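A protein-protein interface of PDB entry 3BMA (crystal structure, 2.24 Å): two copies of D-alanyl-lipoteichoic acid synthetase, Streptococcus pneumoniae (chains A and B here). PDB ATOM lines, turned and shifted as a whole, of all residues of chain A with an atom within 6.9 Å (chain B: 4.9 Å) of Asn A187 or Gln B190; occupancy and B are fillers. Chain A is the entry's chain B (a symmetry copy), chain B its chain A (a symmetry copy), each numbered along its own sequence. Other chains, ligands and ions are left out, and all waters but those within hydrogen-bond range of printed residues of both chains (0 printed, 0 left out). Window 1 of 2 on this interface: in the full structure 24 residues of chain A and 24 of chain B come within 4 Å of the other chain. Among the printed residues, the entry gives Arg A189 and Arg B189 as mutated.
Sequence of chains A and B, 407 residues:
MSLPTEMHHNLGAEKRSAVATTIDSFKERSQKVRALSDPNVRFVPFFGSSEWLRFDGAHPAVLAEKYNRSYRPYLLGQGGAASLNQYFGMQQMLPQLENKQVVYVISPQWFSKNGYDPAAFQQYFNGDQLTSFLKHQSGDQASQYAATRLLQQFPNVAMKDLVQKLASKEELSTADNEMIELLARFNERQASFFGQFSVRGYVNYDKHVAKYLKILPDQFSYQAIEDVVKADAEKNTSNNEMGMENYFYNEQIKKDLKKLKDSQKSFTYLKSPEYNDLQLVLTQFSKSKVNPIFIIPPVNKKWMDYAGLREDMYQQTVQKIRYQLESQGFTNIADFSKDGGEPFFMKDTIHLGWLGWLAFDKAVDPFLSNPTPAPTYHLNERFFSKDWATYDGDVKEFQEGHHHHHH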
ATOM      1  N   ARG A  29       6.411  12.991  30.089  1.00  0.00           N
ATOM      2  CA  ARG A  29       7.451  13.822  30.699  1.00  0.00           C
ATOM      3  C   ARG A  29       7.450  15.254  30.173  1.00  0.00           C
ATOM      4  O   ARG A  29       7.425  16.199  30.958  1.00  0.00           O
ATOM      5  CB  ARG A  29       8.830  13.211  30.459  1.00  0.00           C
ATOM      6  CG  ARG A  29       9.968  13.956  31.124  1.00  0.00           C
ATOM      7  CD  ARG A  29      11.294  13.271  30.877  1.00  0.00           C
ATOM      8  NE  ARG A  29      11.368  11.974  31.547  1.00  0.00           N
ATOM      9  CZ  ARG A  29      11.986  11.758  32.703  1.00  0.00           C
ATOM     10  NH1 ARG A  29      12.604  12.745  33.334  1.00  0.00           N
ATOM     11  NH2 ARG A  29      11.999  10.541  33.224  1.00  0.00           N
ATOM     12  N   ASN A 126       3.450   4.672  32.215  1.00  0.00           N
ATOM     13  CA  ASN A 126       4.248   4.298  31.037  1.00  0.00           C
ATOM     14  C   ASN A 126       5.638   3.766  31.405  1.00  0.00           C
ATOM     15  O   ASN A 126       5.970   3.649  32.591  1.00  0.00           O
ATOM     16  CB  ASN A 126       4.342   5.457  30.026  1.00  0.00           C
ATOM     17  CG  ASN A 126       4.923   6.728  30.626  1.00  0.00           C
ATOM     18  OD1 ASN A 126       5.424   6.733  31.746  1.00  0.00           O
ATOM     19  ND2 ASN A 126       4.869   7.814  29.866  1.00  0.00           N
ATOM     20  N   GLY A 127       6.443   3.450  30.392  1.00  0.00           N
ATOM     21  CA  GLY A 127       7.798   2.964  30.608  1.00  0.00           C
ATOM     22  C   GLY A 127       8.777   4.005  31.118  1.00  0.00           C
ATOM     23  O   GLY A 127       9.740   3.663  31.808  1.00  0.00           O
ATOM     24  N   ASP A 128       8.551   5.269  30.757  1.00  0.00           N
ATOM     25  CA  ASP A 128       9.324   6.385  31.305  1.00  0.00           C
ATOM     26  C   ASP A 128       9.197   6.424  32.823  1.00  0.00           C
ATOM     27  O   ASP A 128      10.201   6.528  33.519  1.00  0.00           O
ATOM     28  CB  ASP A 128       8.877   7.729  30.704  1.00  0.00           C
ATOM     29  CG  ASP A 128       9.880   8.858  30.958  1.00  0.00           C
ATOM     30  OD1 ASP A 128      11.018   8.601  31.427  1.00  0.00           O
ATOM     31  OD2 ASP A 128       9.527  10.020  30.671  1.00  0.00           O
ATOM     32  N   GLN A 129       7.964   6.331  33.316  1.00  0.00           N
ATOM     33  CA  GLN A 129       7.687   6.232  34.749  1.00  0.00           C
ATOM     34  C   GLN A 129       8.340   5.009  35.396  1.00  0.00           C
ATOM     35  O   GLN A 129       8.861   5.106  36.505  1.00  0.00           O
ATOM     36  CB  GLN A 129       6.185   6.211  34.998  1.00  0.00           C
ATOM     37  CG  GLN A 129       5.530   7.581  34.922  1.00  0.00           C
ATOM     38  CD  GLN A 129       4.028   7.500  34.961  1.00  0.00           C
ATOM     39  OE1 GLN A 129       3.461   6.657  35.651  1.00  0.00           O
ATOM     40  NE2 GLN A 129       3.368   8.379  34.215  1.00  0.00           N
ATOM     41  N   LEU A 130       8.316   3.872  34.699  1.00  0.00           N
ATOM     42  CA  LEU A 130       8.973   2.649  35.170  1.00  0.00           C
ATOM     43  C   LEU A 130      10.461   2.903  35.392  1.00  0.00           C
ATOM     44  O   LEU A 130      10.959   2.706  36.500  1.00  0.00           O
ATOM     45  CB  LEU A 130       8.794   1.514  34.160  1.00  0.00           C
ATOM     46  CG  LEU A 130       8.669   0.043  34.582  1.00  0.00           C
ATOM     47  CD1 LEU A 130       9.201  -0.819  33.449  1.00  0.00           C
ATOM     48  CD2 LEU A 130       9.368  -0.321  35.896  1.00  0.00           C
ATOM     49  N   THR A 131      11.152   3.363  34.348  1.00  0.00           N
ATOM     50  CA  THR A 131      12.594   3.588  34.418  1.00  0.00           C
ATOM     51  C   THR A 131      13.013   4.759  35.317  1.00  0.00           C
ATOM     52  O   THR A 131      14.095   4.718  35.900  1.00  0.00           O
ATOM     53  CB  THR A 131      13.236   3.718  33.020  1.00  0.00           C
ATOM     54  OG1 THR A 131      12.521   4.684  32.244  1.00  0.00           O
ATOM     55  CG2 THR A 131      13.225   2.369  32.295  1.00  0.00           C
ATOM     56  N   SER A 132      12.159   5.780  35.434  1.00  0.00           N
ATOM     57  CA  SER A 132      12.396   6.901  36.351  1.00  0.00           C
ATOM     58  C   SER A 132      12.394   6.414  37.788  1.00  0.00           C
ATOM     59  O   SER A 132      13.320   6.705  38.552  1.00  0.00           O
ATOM     60  CB  SER A 132      11.328   7.986  36.200  1.00  0.00           C
ATOM     61  OG  SER A 132      11.429   8.650  34.958  1.00  0.00           O
ATOM     62  N   ALA A 158       7.698  -5.111  32.315  1.00  0.00           N
ATOM     63  CA  ALA A 158       9.023  -4.939  31.730  1.00  0.00           C
ATOM     64  C   ALA A 158      10.054  -4.741  32.847  1.00  0.00           C
ATOM     65  O   ALA A 158       9.756  -4.107  33.861  1.00  0.00           O
ATOM     66  CB  ALA A 158       9.029  -3.757  30.767  1.00  0.00           C
ATOM     67  N   MET A 159      11.245  -5.313  32.665  1.00  0.00           N
ATOM     68  CA  MET A 159      12.326  -5.300  33.675  1.00  0.00           C
ATOM     69  C   MET A 159      11.873  -5.875  35.027  1.00  0.00           C
ATOM     70  O   MET A 159      12.201  -5.344  36.093  1.00  0.00           O
ATOM     71  CB  MET A 159      12.942  -3.898  33.818  1.00  0.00           C
ATOM     72  CG  MET A 159      13.363  -3.271  32.490  1.00  0.00           C
ATOM     73  SD  MET A 159      13.552  -1.487  32.590  1.00  0.00           S
ATOM     74  CE  MET A 159      15.251  -1.384  33.154  1.00  0.00           C
ATOM     75  N   LEU A 182      21.291   3.441  31.640  1.00  0.00           N
ATOM     76  CA  LEU A 182      21.201   3.478  30.183  1.00  0.00           C
ATOM     77  C   LEU A 182      19.763   3.619  29.676  1.00  0.00           C
ATOM     78  O   LEU A 182      19.459   4.533  28.908  1.00  0.00           O
ATOM     79  CB  LEU A 182      21.861   2.223  29.601  1.00  0.00           C
ATOM     80  CG  LEU A 182      21.622   1.691  28.188  1.00  0.00           C
ATOM     81  CD1 LEU A 182      22.058   2.661  27.113  1.00  0.00           C
ATOM     82  CD2 LEU A 182      22.382   0.390  28.054  1.00  0.00           C
ATOM     83  N   LEU A 183      18.884   2.720  30.115  1.00  0.00           N
ATOM     84  CA  LEU A 183      17.515   2.690  29.618  1.00  0.00           C
ATOM     85  C   LEU A 183      16.668   3.860  30.135  1.00  0.00           C
ATOM     86  O   LEU A 183      15.782   4.351  29.426  1.00  0.00           O
ATOM     87  CB  LEU A 183      16.859   1.343  29.934  1.00  0.00           C
ATOM     88  CG  LEU A 183      17.533   0.110  29.316  1.00  0.00           C
ATOM     89  CD1 LEU A 183      16.825  -1.143  29.787  1.00  0.00           C
ATOM     90  CD2 LEU A 183      17.588   0.172  27.780  1.00  0.00           C
ATOM     91  N   ALA A 184      16.957   4.313  31.354  1.00  0.00           N
ATOM     92  CA  ALA A 184      16.300   5.504  31.907  1.00  0.00           C
ATOM     93  C   ALA A 184      16.695   6.771  31.168  1.00  0.00           C
ATOM     94  O   ALA A 184      15.853   7.645  30.947  1.00  0.00           O
ATOM     95  CB  ALA A 184      16.591   5.646  33.392  1.00  0.00           C
ATOM     96  N   ARG A 185      17.974   6.858  30.793  1.00  0.00           N
ATOM     97  CA  ARG A 185      18.512   7.991  30.039  1.00  0.00           C
ATOM     98  C   ARG A 185      17.913   8.007  28.648  1.00  0.00           C
ATOM     99  O   ARG A 185      17.544   9.060  28.143  1.00  0.00           O
ATOM    100  CB  ARG A 185      20.028   7.889  29.912  1.00  0.00           C
ATOM    101  CG  ARG A 185      20.741   9.216  29.727  1.00  0.00           C
ATOM    102  CD  ARG A 185      22.227   9.060  29.334  1.00  0.00           C
ATOM    103  NE  ARG A 185      22.851   7.775  29.693  1.00  0.00           N
ATOM    104  CZ  ARG A 185      23.319   7.442  30.899  1.00  0.00           C
ATOM    105  NH1 ARG A 185      23.224   8.281  31.926  1.00  0.00           N
ATOM    106  NH2 ARG A 185      23.869   6.247  31.082  1.00  0.00           N
ATOM    107  N   PHE A 186      17.829   6.830  28.033  1.00  0.00           N
ATOM    108  CA  PHE A 186      17.219   6.700  26.718  1.00  0.00           C
ATOM    109  C   PHE A 186      15.747   7.106  26.745  1.00  0.00           C
ATOM    110  O   PHE A 186      15.290   7.805  25.848  1.00  0.00           O
ATOM    111  CB  PHE A 186      17.376   5.279  26.169  1.00  0.00           C
ATOM    112  CG  PHE A 186      16.745   5.086  24.825  1.00  0.00           C
ATOM    113  CD1 PHE A 186      17.191   5.813  23.722  1.00  0.00           C
ATOM    114  CD2 PHE A 186      15.702   4.188  24.657  1.00  0.00           C
ATOM    115  CE1 PHE A 186      16.607   5.642  22.481  1.00  0.00           C
ATOM    116  CE2 PHE A 186      15.112   4.010  23.418  1.00  0.00           C
ATOM    117  CZ  PHE A 186      15.566   4.736  22.325  1.00  0.00           C
ATOM    118  N   ASN A 187      15.029   6.695  27.789  1.00  0.00           N
ATOM    119  CA  ASN A 187      13.616   7.031  27.934  1.00  0.00           C
ATOM    120  C   ASN A 187      13.314   8.504  28.152  1.00  0.00           C
ATOM    121  O   ASN A 187      12.298   8.988  27.676  1.00  0.00           O
ATOM    122  CB  ASN A 187      12.953   6.196  29.032  1.00  0.00           C
ATOM    123  CG  ASN A 187      12.105   5.071  28.479  1.00  0.00           C
ATOM    124  OD1 ASN A 187      11.932   4.938  27.267  1.00  0.00           O
ATOM    125  ND2 ASN A 187      11.553   4.261  29.369  1.00  0.00           N
ATOM    126  N   GLU A 188      14.190   9.210  28.866  1.00  0.00           N
ATOM    127  CA  GLU A 188      13.996  10.643  29.087  1.00  0.00           C
ATOM    128  C   GLU A 188      14.342  11.470  27.857  1.00  0.00           C
ATOM    129  O   GLU A 188      13.657  12.447  27.584  1.00  0.00           O
ATOM    130  CB  GLU A 188      14.721  11.165  30.344  1.00  0.00           C
ATOM    131  CG  GLU A 188      16.223  10.960  30.377  1.00  0.00           C
ATOM    132  CD  GLU A 188      16.951  11.971  31.244  1.00  0.00           C
ATOM    133  OE1 GLU A 188      17.934  11.578  31.909  1.00  0.00           O
ATOM    134  OE2 GLU A 188      16.548  13.155  31.258  1.00  0.00           O
ATOM    135  N   ARG A 189      15.379  11.062  27.119  1.00  0.00           N
ATOM    136  CA  ARG A 189      15.767  11.694  25.853  1.00  0.00           C
ATOM    137  C   ARG A 189      14.673  11.511  24.813  1.00  0.00           C
ATOM    138  O   ARG A 189      14.328  12.444  24.091  1.00  0.00           O
ATOM    139  CB  ARG A 189      17.076  11.101  25.321  1.00  0.00           C
ATOM    140  CG  ARG A 189      18.299  11.403  26.173  1.00  0.00           C
ATOM    141  CD  ARG A 189      19.348  12.226  25.449  1.00  0.00           C
ATOM    142  NE  ARG A 189      20.572  12.330  26.247  1.00  0.00           N
ATOM    143  CZ  ARG A 189      21.573  11.449  26.226  1.00  0.00           C
ATOM    144  NH1 ARG A 189      22.638  11.640  26.996  1.00  0.00           N
ATOM    145  NH2 ARG A 189      21.519  10.378  25.443  1.00  0.00           N
ATOM    146  N   GLN A 190      14.131  10.301  24.767  1.00  0.00           N
ATOM    147  CA  GLN A 190      13.077   9.921  23.834  1.00  0.00           C
ATOM    148  C   GLN A 190      11.759  10.630  24.130  1.00  0.00           C
ATOM    149  O   GLN A 190      11.055  11.051  23.209  1.00  0.00           O
ATOM    150  CB  GLN A 190      12.854   8.423  23.955  1.00  0.00           C
ATOM    151  CG  GLN A 190      12.359   7.746  22.733  1.00  0.00           C
ATOM    152  CD  GLN A 190      12.258   6.254  22.927  1.00  0.00           C
ATOM    153  OE1 GLN A 190      12.263   5.501  21.961  1.00  0.00           O
ATOM    154  NE2 GLN A 190      12.161   5.815  24.180  1.00  0.00           N
ATOM    155  N   ALA A 191      11.416  10.723  25.413  1.00  0.00           N
ATOM    156  CA  ALA A 191      10.184  11.383  25.841  1.00  0.00           C
ATOM    157  C   ALA A 191      10.244  12.898  25.674  1.00  0.00           C
ATOM    158  O   ALA A 191       9.268  13.497  25.230  1.00  0.00           O
ATOM    159  CB  ALA A 191       9.845  11.021  27.270  1.00  0.00           C
ATOM    160  N   SER A 192      11.381  13.507  26.016  1.00  0.00           N
ATOM    161  CA  SER A 192      11.502  14.961  25.927  1.00  0.00           C
ATOM    162  C   SER A 192      11.673  15.455  24.495  1.00  0.00           C
ATOM    163  O   SER A 192      11.276  16.575  24.177  1.00  0.00           O
ATOM    164  CB  SER A 192      12.626  15.486  26.824  1.00  0.00           C
ATOM    165  OG  SER A 192      13.863  14.890  26.492  1.00  0.00           O
ATOM    166  N   PHE B 186      14.313  -2.886  23.642  1.00  0.00           N
ATOM    167  CA  PHE B 186      13.700  -2.144  24.738  1.00  0.00           C
ATOM    168  C   PHE B 186      12.418  -1.441  24.319  1.00  0.00           C
ATOM    169  O   PHE B 186      11.393  -1.613  24.965  1.00  0.00           O
ATOM    170  CB  PHE B 186      14.680  -1.137  25.347  1.00  0.00           C
ATOM    171  CG  PHE B 186      14.104  -0.351  26.495  1.00  0.00           C
ATOM    172  CD1 PHE B 186      13.591  -1.002  27.616  1.00  0.00           C
ATOM    173  CD2 PHE B 186      14.076   1.041  26.455  1.00  0.00           C
ATOM    174  CE1 PHE B 186      13.057  -0.281  28.681  1.00  0.00           C
ATOM    175  CE2 PHE B 186      13.548   1.774  27.515  1.00  0.00           C
ATOM    176  CZ  PHE B 186      13.039   1.108  28.632  1.00  0.00           C
ATOM    177  N   ASN B 187      12.482  -0.666  23.238  1.00  0.00           N
ATOM    178  CA  ASN B 187      11.320   0.067  22.735  1.00  0.00           C
ATOM    179  C   ASN B 187      10.134  -0.806  22.324  1.00  0.00           C
ATOM    180  O   ASN B 187       8.995  -0.413  22.528  1.00  0.00           O
ATOM    181  CB  ASN B 187      11.713   0.967  21.572  1.00  0.00           C
ATOM    182  CG  ASN B 187      12.031   2.382  22.006  1.00  0.00           C
ATOM    183  OD1 ASN B 187      11.664   2.822  23.098  1.00  0.00           O
ATOM    184  ND2 ASN B 187      12.705   3.112  21.139  1.00  0.00           N
ATOM    185  N   GLU B 188      10.394  -1.980  21.753  1.00  0.00           N
ATOM    186  CA  GLU B 188       9.300  -2.869  21.362  1.00  0.00           C
ATOM    187  C   GLU B 188       8.666  -3.610  22.532  1.00  0.00           C
ATOM    188  O   GLU B 188       7.463  -3.826  22.530  1.00  0.00           O
ATOM    189  CB  GLU B 188       9.679  -3.818  20.210  1.00  0.00           C
ATOM    190  CG  GLU B 188      10.708  -4.892  20.492  1.00  0.00           C
ATOM    191  CD  GLU B 188      11.028  -5.711  19.247  1.00  0.00           C
ATOM    192  OE1 GLU B 188      12.166  -5.603  18.734  1.00  0.00           O
ATOM    193  OE2 GLU B 188      10.134  -6.445  18.771  1.00  0.00           O
ATOM    194  N   ARG B 189       9.472  -3.976  23.526  1.00  0.00           N
ATOM    195  CA  ARG B 189       8.983  -4.593  24.764  1.00  0.00           C
ATOM    196  C   ARG B 189       8.127  -3.588  25.545  1.00  0.00           C
ATOM    197  O   ARG B 189       7.066  -3.929  26.066  1.00  0.00           O
ATOM    198  CB  ARG B 189      10.175  -5.065  25.613  1.00  0.00           C
ATOM    199  CG  ARG B 189       9.845  -5.518  27.038  1.00  0.00           C
ATOM    200  CD  ARG B 189       9.379  -6.974  27.088  1.00  0.00           C
ATOM    201  NE  ARG B 189       8.932  -7.375  28.423  1.00  0.00           N
ATOM    202  CZ  ARG B 189       7.671  -7.314  28.850  1.00  0.00           C
ATOM    203  NH1 ARG B 189       6.709  -6.862  28.054  1.00  0.00           N
ATOM    204  NH2 ARG B 189       7.370  -7.708  30.080  1.00  0.00           N
ATOM    205  N   GLN B 190       8.607  -2.349  25.593  1.00  0.00           N
ATOM    206  CA  GLN B 190       7.942  -1.220  26.242  1.00  0.00           C
ATOM    207  C   GLN B 190       6.620  -0.866  25.553  1.00  0.00           C
ATOM    208  O   GLN B 190       5.584  -0.776  26.210  1.00  0.00           O
ATOM    209  CB  GLN B 190       8.899  -0.032  26.212  1.00  0.00           C
ATOM    210  CG  GLN B 190       8.516   1.151  27.032  1.00  0.00           C
ATOM    211  CD  GLN B 190       9.685   2.074  27.249  1.00  0.00           C
ATOM    212  OE1 GLN B 190      10.064   2.333  28.384  1.00  0.00           O
ATOM    213  NE2 GLN B 190      10.275   2.567  26.163  1.00  0.00           N
ATOM    214  N   ALA B 191       6.663  -0.694  24.231  1.00  0.00           N
ATOM    215  CA  ALA B 191       5.474  -0.353  23.440  1.00  0.00           C
ATOM    216  C   ALA B 191       4.393  -1.425  23.454  1.00  0.00           C
ATOM    217  O   ALA B 191       3.213  -1.090  23.554  1.00  0.00           O
ATOM    218  CB  ALA B 191       5.847  -0.008  22.011  1.00  0.00           C
ATOM    219  N   SER B 192       4.787  -2.698  23.346  1.00  0.00           N
ATOM    220  CA  SER B 192       3.822  -3.798  23.360  1.00  0.00           C
ATOM    221  C   SER B 192       3.186  -3.981  24.733  1.00  0.00           C
ATOM    222  O   SER B 192       2.013  -4.343  24.829  1.00  0.00           O
ATOM    223  CB  SER B 192       4.457  -5.111  22.890  1.00  0.00           C
ATOM    224  OG  SER B 192       5.453  -5.565  23.793  1.00  0.00           O
ATOM    225  N   PHE B 193       3.960  -3.730  25.792  1.00  0.00           N
ATOM    226  CA  PHE B 193       3.439  -3.887  27.151  1.00  0.00           C
ATOM    227  C   PHE B 193       2.492  -2.766  27.578  1.00  0.00           C
ATOM    228  O   PHE B 193       1.373  -3.047  27.982  1.00  0.00           O
ATOM    229  CB  PHE B 193       4.547  -4.099  28.198  1.00  0.00           C
ATOM    230  CG  PHE B 193       4.015  -4.478  29.556  1.00  0.00           C
ATOM    231  CD1 PHE B 193       3.946  -3.540  30.579  1.00  0.00           C
ATOM    232  CD2 PHE B 193       3.542  -5.764  29.796  1.00  0.00           C
ATOM    233  CE1 PHE B 193       3.430  -3.873  31.821  1.00  0.00           C
ATOM    234  CE2 PHE B 193       3.025  -6.112  31.039  1.00  0.00           C
ATOM    235  CZ  PHE B 193       2.967  -5.166  32.052  1.00  0.00           C
ATOM    236  N   PHE B 194       2.934  -1.511  27.488  1.00  0.00           N
ATOM    237  CA  PHE B 194       2.128  -0.375  27.973  1.00  0.00           C
ATOM    238  C   PHE B 194       1.122   0.172  26.960  1.00  0.00           C
ATOM    239  O   PHE B 194       0.117   0.778  27.346  1.00  0.00           O
ATOM    240  CB  PHE B 194       3.020   0.753  28.514  1.00  0.00           C
ATOM    241  CG  PHE B 194       3.947   0.313  29.612  1.00  0.00           C
ATOM    242  CD1 PHE B 194       5.307   0.145  29.365  1.00  0.00           C
ATOM    243  CD2 PHE B 194       3.458   0.037  30.886  1.00  0.00           C
ATOM    244  CE1 PHE B 194       6.166  -0.286  30.369  1.00  0.00           C
ATOM    245  CE2 PHE B 194       4.307  -0.391  31.895  1.00  0.00           C
ATOM    246  CZ  PHE B 194       5.666  -0.550  31.640  1.00  0.00           C
ATOM    247  N   GLY B 195       1.378  -0.055  25.675  1.00  0.00           N
ATOM    248  CA  GLY B 195       0.482   0.412  24.615  1.00  0.00           C
ATOM    249  C   GLY B 195      -0.825  -0.352  24.511  1.00  0.00           C
ATOM    250  O   GLY B 195      -1.742   0.076  23.808  1.00  0.00           O
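ND2 of Asn B187 is in hydrogen-bond range of OE1 of Gln A190, at 2.6 Å.
The side-chain amide oxygen of Gln B190 lies within hydrogen-bond range of the side-chain amide nitrogen of Asn A187 (2.6 Å).
The guanidinium group (NH2) of Arg B189 sits close to the backbone NH (N) of Ala A158 (3.4 Å).
O of Arg B189 sits at hydrogen-bond distance from OG of Ser B192 (3.2 Å).
OG1 of Thr A131 is in hydrogen-bond range of O of Gly A127.
The side-chain amide nitrogen of Asn A187 sits at hydrogen-bond distance from the backbone carbonyl oxygen of Gly A127.
The backbone NH of Asp A128 lies close to the side-chain amide nitrogen of Asn A187 (3.5 Å).
OG1 of Thr A131 is in hydrogen-bond range of ND2 of Asn A187, at 3.1 Å.
The side-chain amide nitrogen of Gln A190 lies within hydrogen-bond range of the side-chain amide oxygen of Asn A187 (3.2 Å).
Among the printed residues, pairs that only touch across the chains: Gly A127 with Gln B190 (3.2 Å), Phe A186 with Asn B187 (3.4 Å), Asn A187 with Phe B186 (3.6 Å), Gly A127 with Phe B194 (3.6 Å), Leu A183 with Phe B186 (3.8 Å), Thr A131 with Phe B186 (3.9 Å), Phe A186 with Phe B186 (3.97 Å) and Leu A130 with Phe B194 (3.98 Å).
Of the printed residues of chain B, Leu A130 touches Phe B194 (3.98 Å).
Of the printed residues of chain B, Leu A183 touches Phe B186.
Gln B190 touches just these residues of chain A: Gly A127 and Asn A187.
The nearest residue of chain B that does not touch Asn A187 is Asn B187 (4.7 Å).
Of the 21 printed residues of chain A, 8 touch a printed residue of chain B.
Hydrophobic or aromatic side chains of chain A within 4 Å of the printed part of chain B: Leu A130, Leu A183 and Phe A186.
Hydrophobic or aromatic side chains of chain B that line the printed part of chain A: Phe B186 and Phe B194.
Among the printed residues, no Asp or Glu carboxylate lies within 4 Å of a Lys or Arg side-chain nitrogen of the other chain.
Phe B186 touches its own counterpart, Phe A186.
Phe A186 touches Asn B187, and with the chains exchanged Asn A187 touches Phe B186.
Asn A187 touches Gln B190, and with the chains exchanged Gln A190 touches Asn B187.
Positions printed for both chains: 186, 187, 188, 189, 190, 191 and 192.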
